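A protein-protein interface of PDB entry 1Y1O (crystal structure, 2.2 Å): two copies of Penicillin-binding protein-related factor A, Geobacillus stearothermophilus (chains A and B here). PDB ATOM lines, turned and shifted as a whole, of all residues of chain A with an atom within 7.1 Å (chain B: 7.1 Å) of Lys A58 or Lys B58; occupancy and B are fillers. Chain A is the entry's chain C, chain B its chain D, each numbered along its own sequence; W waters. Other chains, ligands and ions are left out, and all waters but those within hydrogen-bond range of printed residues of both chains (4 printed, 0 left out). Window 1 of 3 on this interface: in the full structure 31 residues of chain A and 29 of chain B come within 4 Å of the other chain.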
ATOM      1  N   HIS A  56      15.062 -21.222   5.036  1.00  0.00           N
ATOM      2  CA  HIS A  56      15.382 -21.113   6.443  1.00  0.00           C
ATOM      3  C   HIS A  56      14.239 -21.642   7.259  1.00  0.00           C
ATOM      4  O   HIS A  56      13.079 -21.530   6.871  1.00  0.00           O
ATOM      5  CB  HIS A  56      15.618 -19.637   6.830  1.00  0.00           C
ATOM      6  CG  HIS A  56      16.893 -19.066   6.290  1.00  0.00           C
ATOM      7  ND1 HIS A  56      18.080 -19.094   7.001  1.00  0.00           N
ATOM      8  CD2 HIS A  56      17.172 -18.461   5.114  1.00  0.00           C
ATOM      9  CE1 HIS A  56      19.028 -18.507   6.292  1.00  0.00           C
ATOM     10  NE2 HIS A  56      18.504 -18.117   5.140  1.00  0.00           N
ATOM     11  N   LYS A  57      14.585 -22.203   8.413  1.00  0.00           N
ATOM     12  CA  LYS A  57      13.595 -22.534   9.418  1.00  0.00           C
ATOM     13  C   LYS A  57      13.141 -21.242  10.098  1.00  0.00           C
ATOM     14  O   LYS A  57      13.942 -20.382  10.384  1.00  0.00           O
ATOM     15  CB  LYS A  57      14.165 -23.525  10.444  1.00  0.00           C
ATOM     16  CG  LYS A  57      13.060 -24.111  11.300  1.00  0.00           C
ATOM     17  CD  LYS A  57      13.564 -25.070  12.357  1.00  0.00           C
ATOM     18  CE  LYS A  57      12.385 -25.688  13.072  1.00  0.00           C
ATOM     19  NZ  LYS A  57      11.743 -24.700  13.974  1.00  0.00           N
ATOM     20  N   LYS A  58      11.850 -21.086  10.305  1.00  0.00           N
ATOM     21  CA  LYS A  58      11.347 -20.028  11.154  1.00  0.00           C
ATOM     22  C   LYS A  58      11.575 -20.362  12.641  1.00  0.00           C
ATOM     23  O   LYS A  58      11.366 -21.503  13.047  1.00  0.00           O
ATOM     24  CB  LYS A  58       9.862 -19.822  10.870  1.00  0.00           C
ATOM     25  CG  LYS A  58       9.591 -18.968   9.644  1.00  0.00           C
ATOM     26  CD  LYS A  58       8.214 -19.210   9.116  1.00  0.00           C
ATOM     27  CE  LYS A  58       7.533 -17.909   8.655  1.00  0.00           C
ATOM     28  NZ  LYS A  58       8.229 -17.190   7.591  1.00  0.00           N
ATOM     29  N   PRO A  59      12.003 -19.369  13.451  1.00  0.00           N
ATOM     30  CA  PRO A  59      12.083 -19.513  14.916  1.00  0.00           C
ATOM     31  C   PRO A  59      10.724 -19.772  15.554  1.00  0.00           C
ATOM     32  O   PRO A  59       9.729 -19.181  15.123  1.00  0.00           O
ATOM     33  CB  PRO A  59      12.595 -18.151  15.384  1.00  0.00           C
ATOM     34  CG  PRO A  59      13.178 -17.506  14.214  1.00  0.00           C
ATOM     35  CD  PRO A  59      12.462 -18.041  13.004  1.00  0.00           C
ATOM     36  N   THR A  60      10.680 -20.638  16.572  1.00  0.00           N
ATOM     37  CA  THR A  60       9.426 -20.878  17.309  1.00  0.00           C
ATOM     38  C   THR A  60       9.084 -19.593  18.029  1.00  0.00           C
ATOM     39  O   THR A  60       9.949 -19.007  18.672  1.00  0.00           O
ATOM     40  CB  THR A  60       9.533 -22.027  18.353  1.00  0.00           C
ATOM     41  OG1 THR A  60      10.390 -23.055  17.848  1.00  0.00           O
ATOM     42  CG2 THR A  60       8.133 -22.644  18.645  1.00  0.00           C
ATOM     43  N   PRO A  61       7.833 -19.115  17.880  1.00  0.00           N
ATOM     44  CA  PRO A  61       7.460 -17.898  18.590  1.00  0.00           C
ATOM     45  C   PRO A  61       7.359 -18.144  20.107  1.00  0.00           C
ATOM     46  O   PRO A  61       6.874 -19.197  20.554  1.00  0.00           O
ATOM     47  CB  PRO A  61       6.098 -17.527  17.992  1.00  0.00           C
ATOM     48  CG  PRO A  61       5.575 -18.785  17.409  1.00  0.00           C
ATOM     49  CD  PRO A  61       6.731 -19.666  17.079  1.00  0.00           C
ATOM     50  N   THR A  87       2.227 -19.777  11.063  1.00  0.00           N
ATOM     51  CA  THR A  87       2.718 -20.292   9.763  1.00  0.00           C
ATOM     52  C   THR A  87       3.425 -21.659   9.884  1.00  0.00           C
ATOM     53  O   THR A  87       3.730 -22.139  10.988  1.00  0.00           O
ATOM     54  CB  THR A  87       3.662 -19.292   9.068  1.00  0.00           C
ATOM     55  OG1 THR A  87       4.968 -19.405   9.608  1.00  0.00           O
ATOM     56  CG2 THR A  87       3.218 -17.851   9.257  1.00  0.00           C
ATOM     57  N   THR A  88       3.701 -22.271   8.737  1.00  0.00           N
ATOM     58  CA  THR A  88       4.568 -23.437   8.659  1.00  0.00           C
ATOM     59  C   THR A  88       5.994 -23.051   8.978  1.00  0.00           C
ATOM     60  O   THR A  88       6.340 -21.875   8.966  1.00  0.00           O
ATOM     61  CB  THR A  88       4.577 -24.022   7.245  1.00  0.00           C
ATOM     62  OG1 THR A  88       4.922 -22.980   6.322  1.00  0.00           O
ATOM     63  CG2 THR A  88       3.210 -24.622   6.931  1.00  0.00           C
ATOM     64  N   ASP A  89       6.823 -24.056   9.200  1.00  0.00           N
ATOM     65  CA  ASP A  89       8.145 -23.888   9.773  1.00  0.00           C
ATOM     66  C   ASP A  89       9.242 -23.515   8.790  1.00  0.00           C
ATOM     67  O   ASP A  89      10.255 -22.985   9.199  1.00  0.00           O
ATOM     68  CB  ASP A  89       8.558 -25.172  10.529  1.00  0.00           C
ATOM     69  CG  ASP A  89       8.027 -25.222  11.976  1.00  0.00           C
ATOM     70  OD1 ASP A  89       7.612 -24.167  12.540  1.00  0.00           O
ATOM     71  OD2 ASP A  89       8.055 -26.331  12.570  1.00  0.00           O
ATOM     72  N   TYR A  90       9.089 -23.801   7.511  1.00  0.00           N
ATOM     73  CA  TYR A  90      10.183 -23.463   6.566  1.00  0.00           C
ATOM     74  C   TYR A  90       9.700 -22.655   5.391  1.00  0.00           C
ATOM     75  O   TYR A  90       8.688 -22.988   4.781  1.00  0.00           O
ATOM     76  CB  TYR A  90      10.881 -24.719   6.035  1.00  0.00           C
ATOM     77  CG  TYR A  90      11.543 -25.578   7.080  1.00  0.00           C
ATOM     78  CD1 TYR A  90      12.910 -25.503   7.319  1.00  0.00           C
ATOM     79  CD2 TYR A  90      10.795 -26.500   7.815  1.00  0.00           C
ATOM     80  CE1 TYR A  90      13.517 -26.351   8.252  1.00  0.00           C
ATOM     81  CE2 TYR A  90      11.367 -27.310   8.754  1.00  0.00           C
ATOM     82  CZ  TYR A  90      12.728 -27.246   8.975  1.00  0.00           C
ATOM     83  OH  TYR A  90      13.266 -28.089   9.944  1.00  0.00           O
ATOM     84  N   ASN A  91      10.426 -21.601   5.053  1.00  0.00           N
ATOM     85  CA  ASN A  91      10.162 -20.946   3.780  1.00  0.00           C
ATOM     86  C   ASN A  91      11.412 -20.378   3.114  1.00  0.00           C
ATOM     87  O   ASN A  91      12.505 -20.401   3.689  1.00  0.00           O
ATOM     88  CB  ASN A  91       8.975 -19.940   3.860  1.00  0.00           C
ATOM     89  CG  ASN A  91       9.336 -18.613   4.543  1.00  0.00           C
ATOM     90  OD1 ASN A  91      10.403 -18.480   5.146  1.00  0.00           O
ATOM     91  ND2 ASN A  91       8.439 -17.625   4.448  1.00  0.00           N
ATOM     92  N   GLY A  92      11.257 -19.844   1.912  1.00  0.00           N
ATOM     93  CA  GLY A  92      12.383 -19.258   1.201  1.00  0.00           C
ATOM     94  C   GLY A  92      12.073 -19.224  -0.286  1.00  0.00           C
ATOM     95  O   GLY A  92      10.916 -19.218  -0.686  1.00  0.00           O
ATOM     96  N   TYR A  98       8.339 -18.730  -4.502  1.00  0.00           N
ATOM     97  CA  TYR A  98       8.109 -18.947  -3.083  1.00  0.00           C
ATOM     98  C   TYR A  98       7.946 -20.431  -2.752  1.00  0.00           C
ATOM     99  O   TYR A  98       7.121 -21.111  -3.364  1.00  0.00           O
ATOM    100  CB  TYR A  98       6.878 -18.170  -2.633  1.00  0.00           C
ATOM    101  CG  TYR A  98       6.629 -18.263  -1.156  1.00  0.00           C
ATOM    102  CD1 TYR A  98       7.379 -17.519  -0.241  1.00  0.00           C
ATOM    103  CD2 TYR A  98       5.666 -19.108  -0.667  1.00  0.00           C
ATOM    104  CE1 TYR A  98       7.114 -17.602   1.109  1.00  0.00           C
ATOM    105  CE2 TYR A  98       5.439 -19.208   0.654  1.00  0.00           C
ATOM    106  CZ  TYR A  98       6.127 -18.444   1.545  1.00  0.00           C
ATOM    107  OH  TYR A  98       5.818 -18.590   2.894  1.00  0.00           O
ATOM    108  N   ASP A 100       7.445 -23.153   0.566  1.00  0.00           N
ATOM    109  CA  ASP A 100       7.005 -23.148   1.936  1.00  0.00           C
ATOM    110  C   ASP A 100       6.724 -24.588   2.330  1.00  0.00           C
ATOM    111  O   ASP A 100       6.163 -25.330   1.550  1.00  0.00           O
ATOM    112  CB  ASP A 100       5.760 -22.272   2.027  1.00  0.00           C
ATOM    113  CG  ASP A 100       5.240 -22.079   3.447  1.00  0.00           C
ATOM    114  OD1 ASP A 100       4.774 -23.080   4.043  1.00  0.00           O
ATOM    115  OD2 ASP A 100       5.210 -20.901   3.940  1.00  0.00           O
ATOM    116  N   HIS A 124      -2.540 -21.542   6.889  1.00  0.00           N
ATOM    117  CA  HIS A 124      -1.391 -20.907   6.194  1.00  0.00           C
ATOM    118  C   HIS A 124      -1.047 -21.555   4.831  1.00  0.00           C
ATOM    119  O   HIS A 124      -0.892 -20.867   3.818  1.00  0.00           O
ATOM    120  CB  HIS A 124      -0.125 -20.903   7.088  1.00  0.00           C
ATOM    121  CG  HIS A 124       1.056 -20.259   6.417  1.00  0.00           C
ATOM    122  ND1 HIS A 124       1.138 -18.897   6.211  1.00  0.00           N
ATOM    123  CD2 HIS A 124       2.147 -20.794   5.828  1.00  0.00           C
ATOM    124  CE1 HIS A 124       2.250 -18.617   5.558  1.00  0.00           C
ATOM    125  NE2 HIS A 124       2.893 -19.749   5.337  1.00  0.00           N
ATOM    126  N   HIS B  56       4.455 -12.118   6.952  1.00  0.00           N
ATOM    127  CA  HIS B  56       4.545 -12.144   8.436  1.00  0.00           C
ATOM    128  C   HIS B  56       5.867 -11.557   8.881  1.00  0.00           C
ATOM    129  O   HIS B  56       6.855 -11.671   8.181  1.00  0.00           O
ATOM    130  CB  HIS B  56       4.431 -13.575   9.004  1.00  0.00           C
ATOM    131  CG  HIS B  56       3.086 -14.182   8.816  1.00  0.00           C
ATOM    132  ND1 HIS B  56       2.065 -14.015   9.728  1.00  0.00           N
ATOM    133  CD2 HIS B  56       2.555 -14.861   7.770  1.00  0.00           C
ATOM    134  CE1 HIS B  56       0.981 -14.625   9.283  1.00  0.00           C
ATOM    135  NE2 HIS B  56       1.258 -15.155   8.101  1.00  0.00           N
ATOM    136  N   LYS B  57       5.868 -10.905  10.040  1.00  0.00           N
ATOM    137  CA  LYS B  57       7.128 -10.633  10.717  1.00  0.00           C
ATOM    138  C   LYS B  57       7.710 -11.936  11.283  1.00  0.00           C
ATOM    139  O   LYS B  57       6.998 -12.720  11.894  1.00  0.00           O
ATOM    140  CB  LYS B  57       6.940  -9.604  11.810  1.00  0.00           C
ATOM    141  CG  LYS B  57       8.251  -9.113  12.377  1.00  0.00           C
ATOM    142  CD  LYS B  57       8.027  -7.988  13.365  1.00  0.00           C
ATOM    143  CE  LYS B  57       9.335  -7.246  13.601  1.00  0.00           C
ATOM    144  NZ  LYS B  57      10.452  -8.129  14.077  1.00  0.00           N
ATOM    145  N   LYS B  58       8.992 -12.189  11.056  1.00  0.00           N
ATOM    146  CA  LYS B  58       9.620 -13.378  11.635  1.00  0.00           C
ATOM    147  C   LYS B  58       9.694 -13.231  13.143  1.00  0.00           C
ATOM    148  O   LYS B  58      10.049 -12.150  13.633  1.00  0.00           O
ATOM    149  CB  LYS B  58      11.024 -13.603  11.093  1.00  0.00           C
ATOM    150  CG  LYS B  58      11.066 -14.076   9.661  1.00  0.00           C
ATOM    151  CD  LYS B  58      12.437 -14.649   9.366  1.00  0.00           C
ATOM    152  CE  LYS B  58      12.426 -16.190   9.333  1.00  0.00           C
ATOM    153  NZ  LYS B  58      12.044 -16.707   7.966  1.00  0.00           N
ATOM    154  N   PRO B  59       9.326 -14.301  13.886  1.00  0.00           N
ATOM    155  CA  PRO B  59       9.368 -14.183  15.337  1.00  0.00           C
ATOM    156  C   PRO B  59      10.796 -13.902  15.837  1.00  0.00           C
ATOM    157  O   PRO B  59      11.772 -14.308  15.184  1.00  0.00           O
ATOM    158  CB  PRO B  59       8.848 -15.536  15.825  1.00  0.00           C
ATOM    159  CG  PRO B  59       8.113 -16.124  14.647  1.00  0.00           C
ATOM    160  CD  PRO B  59       8.849 -15.628  13.449  1.00  0.00           C
ATOM    161  N   THR B  60      10.900 -13.161  16.941  1.00  0.00           N
ATOM    162  CA  THR B  60      12.192 -12.930  17.610  1.00  0.00           C
ATOM    163  C   THR B  60      12.903 -14.293  17.833  1.00  0.00           C
ATOM    164  O   THR B  60      12.268 -15.252  18.327  1.00  0.00           O
ATOM    165  CB  THR B  60      11.980 -12.180  18.950  1.00  0.00           C
ATOM    166  OG1 THR B  60      11.096 -11.065  18.738  1.00  0.00           O
ATOM    167  CG2 THR B  60      13.318 -11.686  19.566  1.00  0.00           C
ATOM    168  N   PRO B  61      14.196 -14.404  17.445  1.00  0.00           N
ATOM    169  CA  PRO B  61      14.882 -15.698  17.590  1.00  0.00           C
ATOM    170  C   PRO B  61      15.485 -15.951  18.980  1.00  0.00           C
ATOM    171  O   PRO B  61      16.175 -15.104  19.554  1.00  0.00           O
ATOM    172  CB  PRO B  61      15.989 -15.653  16.521  1.00  0.00           C
ATOM    173  CG  PRO B  61      16.095 -14.210  16.113  1.00  0.00           C
ATOM    174  CD  PRO B  61      15.096 -13.384  16.880  1.00  0.00           C
ATOM    175  N   ALA B  85      19.718 -12.837  14.707  1.00  0.00           N
ATOM    176  CA  ALA B  85      18.996 -13.253  13.505  1.00  0.00           C
ATOM    177  C   ALA B  85      19.957 -13.389  12.320  1.00  0.00           C
ATOM    178  O   ALA B  85      20.812 -12.509  12.083  1.00  0.00           O
ATOM    179  CB  ALA B  85      17.851 -12.269  13.183  1.00  0.00           C
ATOM    180  N   THR B  87      18.793 -13.634   9.363  1.00  0.00           N
ATOM    181  CA  THR B  87      17.952 -13.213   8.246  1.00  0.00           C
ATOM    182  C   THR B  87      17.244 -11.887   8.571  1.00  0.00           C
ATOM    183  O   THR B  87      17.229 -11.457   9.729  1.00  0.00           O
ATOM    184  CB  THR B  87      16.932 -14.335   7.880  1.00  0.00           C
ATOM    185  OG1 THR B  87      16.196 -13.952   6.720  1.00  0.00           O
ATOM    186  CG2 THR B  87      15.937 -14.574   8.988  1.00  0.00           C
ATOM    187  N   THR B  88      16.666 -11.258   7.546  1.00  0.00           N
ATOM    188  CA  THR B  88      15.830 -10.055   7.683  1.00  0.00           C
ATOM    189  C   THR B  88      14.494 -10.376   8.369  1.00  0.00           C
ATOM    190  O   THR B  88      14.145 -11.531   8.504  1.00  0.00           O
ATOM    191  CB  THR B  88      15.504  -9.461   6.298  1.00  0.00           C
ATOM    192  OG1 THR B  88      14.938 -10.496   5.484  1.00  0.00           O
ATOM    193  CG2 THR B  88      16.763  -8.874   5.617  1.00  0.00           C
ATOM    194  N   ASP B  89      13.734  -9.341   8.738  1.00  0.00           N
ATOM    195  CA  ASP B  89      12.577  -9.467   9.618  1.00  0.00           C
ATOM    196  C   ASP B  89      11.201  -9.826   9.035  1.00  0.00           C
ATOM    197  O   ASP B  89      10.368 -10.354   9.777  1.00  0.00           O
ATOM    198  CB  ASP B  89      12.408  -8.166  10.391  1.00  0.00           C
ATOM    199  CG  ASP B  89      13.525  -7.926  11.401  1.00  0.00           C
ATOM    200  OD1 ASP B  89      14.416  -8.810  11.564  1.00  0.00           O
ATOM    201  OD2 ASP B  89      13.502  -6.837  12.026  1.00  0.00           O
ATOM    202  N   TYR B  90      10.935  -9.489   7.769  1.00  0.00           N
ATOM    203  CA  TYR B  90       9.640  -9.789   7.136  1.00  0.00           C
ATOM    204  C   TYR B  90       9.811 -10.683   5.910  1.00  0.00           C
ATOM    205  O   TYR B  90      10.730 -10.493   5.152  1.00  0.00           O
ATOM    206  CB  TYR B  90       8.940  -8.499   6.688  1.00  0.00           C
ATOM    207  CG  TYR B  90       8.707  -7.532   7.811  1.00  0.00           C
ATOM    208  CD1 TYR B  90       7.507  -7.548   8.511  1.00  0.00           C
ATOM    209  CD2 TYR B  90       9.709  -6.628   8.207  1.00  0.00           C
ATOM    210  CE1 TYR B  90       7.302  -6.681   9.591  1.00  0.00           C
ATOM    211  CE2 TYR B  90       9.512  -5.754   9.276  1.00  0.00           C
ATOM    212  CZ  TYR B  90       8.280  -5.780   9.948  1.00  0.00           C
ATOM    213  OH  TYR B  90       8.031  -4.947  11.013  1.00  0.00           O
ATOM    214  N   ASN B  91       8.928 -11.665   5.754  1.00  0.00           N
ATOM    215  CA  ASN B  91       8.820 -12.410   4.511  1.00  0.00           C
ATOM    216  C   ASN B  91       7.444 -12.993   4.254  1.00  0.00           C
ATOM    217  O   ASN B  91       6.625 -13.071   5.161  1.00  0.00           O
ATOM    218  CB  ASN B  91       9.964 -13.433   4.299  1.00  0.00           C
ATOM    219  CG  ASN B  91       9.848 -14.720   5.153  1.00  0.00           C
ATOM    220  OD1 ASN B  91       8.775 -15.139   5.634  1.00  0.00           O
ATOM    221  ND2 ASN B  91      10.982 -15.397   5.270  1.00  0.00           N
ATOM    222  N   GLY B  92       7.196 -13.362   2.991  1.00  0.00           N
ATOM    223  CA  GLY B  92       5.980 -14.029   2.612  1.00  0.00           C
ATOM    224  C   GLY B  92       5.889 -14.173   1.107  1.00  0.00           C
ATOM    225  O   GLY B  92       6.918 -14.146   0.419  1.00  0.00           O
ATOM    226  N   TYR B  98       8.546 -14.743  -3.796  1.00  0.00           N
ATOM    227  CA  TYR B  98       8.992 -14.622  -2.445  1.00  0.00           C
ATOM    228  C   TYR B  98       9.323 -13.151  -2.210  1.00  0.00           C
ATOM    229  O   TYR B  98      10.070 -12.554  -2.975  1.00  0.00           O
ATOM    230  CB  TYR B  98      10.210 -15.523  -2.254  1.00  0.00           C
ATOM    231  CG  TYR B  98      10.916 -15.344  -0.957  1.00  0.00           C
ATOM    232  CD1 TYR B  98      10.449 -15.969   0.201  1.00  0.00           C
ATOM    233  CD2 TYR B  98      12.085 -14.538  -0.870  1.00  0.00           C
ATOM    234  CE1 TYR B  98      11.129 -15.822   1.423  1.00  0.00           C
ATOM    235  CE2 TYR B  98      12.747 -14.391   0.351  1.00  0.00           C
ATOM    236  CZ  TYR B  98      12.259 -15.014   1.489  1.00  0.00           C
ATOM    237  OH  TYR B  98      12.935 -14.886   2.697  1.00  0.00           O
ATOM    238  N   ASP B 100      10.660 -10.349   0.655  1.00  0.00           N
ATOM    239  CA  ASP B 100      11.556 -10.379   1.810  1.00  0.00           C
ATOM    240  C   ASP B 100      12.029  -8.943   2.037  1.00  0.00           C
ATOM    241  O   ASP B 100      12.488  -8.276   1.109  1.00  0.00           O
ATOM    242  CB  ASP B 100      12.694 -11.374   1.523  1.00  0.00           C
ATOM    243  CG  ASP B 100      13.717 -11.483   2.647  1.00  0.00           C
ATOM    244  OD1 ASP B 100      14.301 -10.456   3.032  1.00  0.00           O
ATOM    245  OD2 ASP B 100      14.018 -12.609   3.099  1.00  0.00           O
ATOM    246  N   HIS B 124      22.255 -12.256   3.477  1.00  0.00           N
ATOM    247  CA  HIS B 124      21.006 -12.981   3.245  1.00  0.00           C
ATOM    248  C   HIS B 124      20.261 -12.402   2.025  1.00  0.00           C
ATOM    249  O   HIS B 124      19.852 -13.162   1.140  1.00  0.00           O
ATOM    250  CB  HIS B 124      20.107 -12.964   4.488  1.00  0.00           C
ATOM    251  CG  HIS B 124      18.686 -13.361   4.203  1.00  0.00           C
ATOM    252  ND1 HIS B 124      18.305 -14.668   3.978  1.00  0.00           N
ATOM    253  CD2 HIS B 124      17.565 -12.617   4.064  1.00  0.00           C
ATOM    254  CE1 HIS B 124      17.006 -14.715   3.742  1.00  0.00           C
ATOM    255  NE2 HIS B 124      16.533 -13.483   3.791  1.00  0.00           N
HETATM  256  O   HOH W   1      13.297 -17.809   4.622  1.00  0.00           O
HETATM  257  O   HOH W   2      -0.783 -16.957   7.000  1.00  0.00           O
HETATM  258  O   HOH W   3       5.632 -15.578   6.107  1.00  0.00           O
HETATM  259  O   HOH W   4      20.138 -16.400   3.990  1.00  0.00           O
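Of chain B, only Lys B58 and Asn B91 come within 4 Å of Lys A58. Lys B58 touches two residues of chain A. Printed residues of chain B within 4 Å of Gly A92: Tyr B98. Of the printed residues of chain B, Pro A59 touches Pro B59 (3.5 Å). Of the printed residues of chain B, Tyr A98 touches Gly B92 (3.5 Å) and Tyr B98 (3.5 Å). Printed residues of chain A within 4 Å of Pro B59: Pro A59 and Pro A61. Of the printed residues of chain B, His A56 touches His B124. The nearest residue of chain A that does not touch Lys B58 is Pro A59 (4.1 Å). The nearest printed residue of chain B that does not touch Asn A91 is Tyr B98 (4.4 Å).
The backbone NH (N) of Lys B58 sits at hydrogen-bond distance from the backbone carbonyl oxygen (O) of Asp B89, at 2.6 Å. The side-chain carboxylate of Asp A100 is in hydrogen-bond range of the side-chain hydroxyl of Tyr A98, at 2.6 Å. The backbone NH (N) of His A56 sits at hydrogen-bond distance from the backbone carbonyl oxygen (O) of Asn A91 (3.0 Å). O of Asn B91 is in hydrogen-bond range of N of His B56. The side-chain amide nitrogen (ND2) of Asn A91 is in hydrogen-bond range of the side-chain hydroxyl (OH) of Tyr A98, 3.2 Å away. The side-chain carboxylate (OD2) of Asp B100 lies within hydrogen-bond range of a ring nitrogen (NE2) of His B124 (2.8 Å).
Among the printed residues, merely in contact across the chains: Gly A92 with Tyr B98 (3.4 Å), Thr A87 with His B56 (3.4 Å), Tyr A98 with Tyr B98 (3.5 Å), Tyr A98 with Gly B92 (3.5 Å), Pro A59 with Pro B59 (3.5 Å), His A56 with His B124 (3.6 Å), Asn A91 with Lys B58 (3.7 Å), Lys A58 with Lys B58 (3.7 Å) and Pro A61 with Pro B59 (3.9 Å).
The side-chain amide oxygen of Asn B91 lies within hydrogen-bond range of the side-chain amide nitrogen of Asn A91. The side-chain amide oxygen of Asn B91 is in hydrogen-bond range of the side-chain amino group of Lys A58 (2.9 Å).
Of the 16 printed residues of chain B, 7 touch a printed residue of chain A. Printed residues of chain B that touch a printed residue of chain A: His B56, Lys B58, Pro B59, Asn B91, Gly B92, Tyr B98 and His B124. Along chain B the printed residues that touch a printed residue of chain A span positions 56 to 124. Of the 15 printed residues of chain A, 8 touch a printed residue of chain B. Printed residues of chain A that touch a printed residue of chain B: His A56, Lys A58, Pro A59, Pro A61, Thr A87, Asn A91, Gly A92 and Tyr A98. Among the printed residues, no Asp or Glu carboxylate lies within 4 Å of a Lys or Arg side-chain nitrogen of the other chain.
Lys A58 touches Asn B91, and with the chains exchanged Asn A91 touches Lys B58. Pro A59 touches its own counterpart, Pro B59. Gly A92 touches Tyr B98, and with the chains exchanged Tyr A98 touches Gly B92. Tyr B98 touches its own counterpart, Tyr A98. Positions printed for both chains: 56, 57, 58, 59, 60, 61, 87, 88, 89, 90, 91, 92, 98, 100 and 124. Of the 11 pairs that touch across the chains among the printed residues, 8 have their exchanged pair printed and touching as well.
Water W4 bridges a ring nitrogen (ND1) of His B124 and a ring nitrogen (NE2) of His A56. Water W2 bridges a ring nitrogen (ND1) of His A124 (2.8 Å) and a ring nitrogen (NE2) of His B56 (2.9 Å). Water W3 bridges O of Asn B91 (2.9 Å) and NZ of Lys A58 (3.4 Å). Water W1 lies within hydrogen-bond range of O of Asn A91 (2.9 Å) and ND2 of Asn B91 (3.4 Å).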
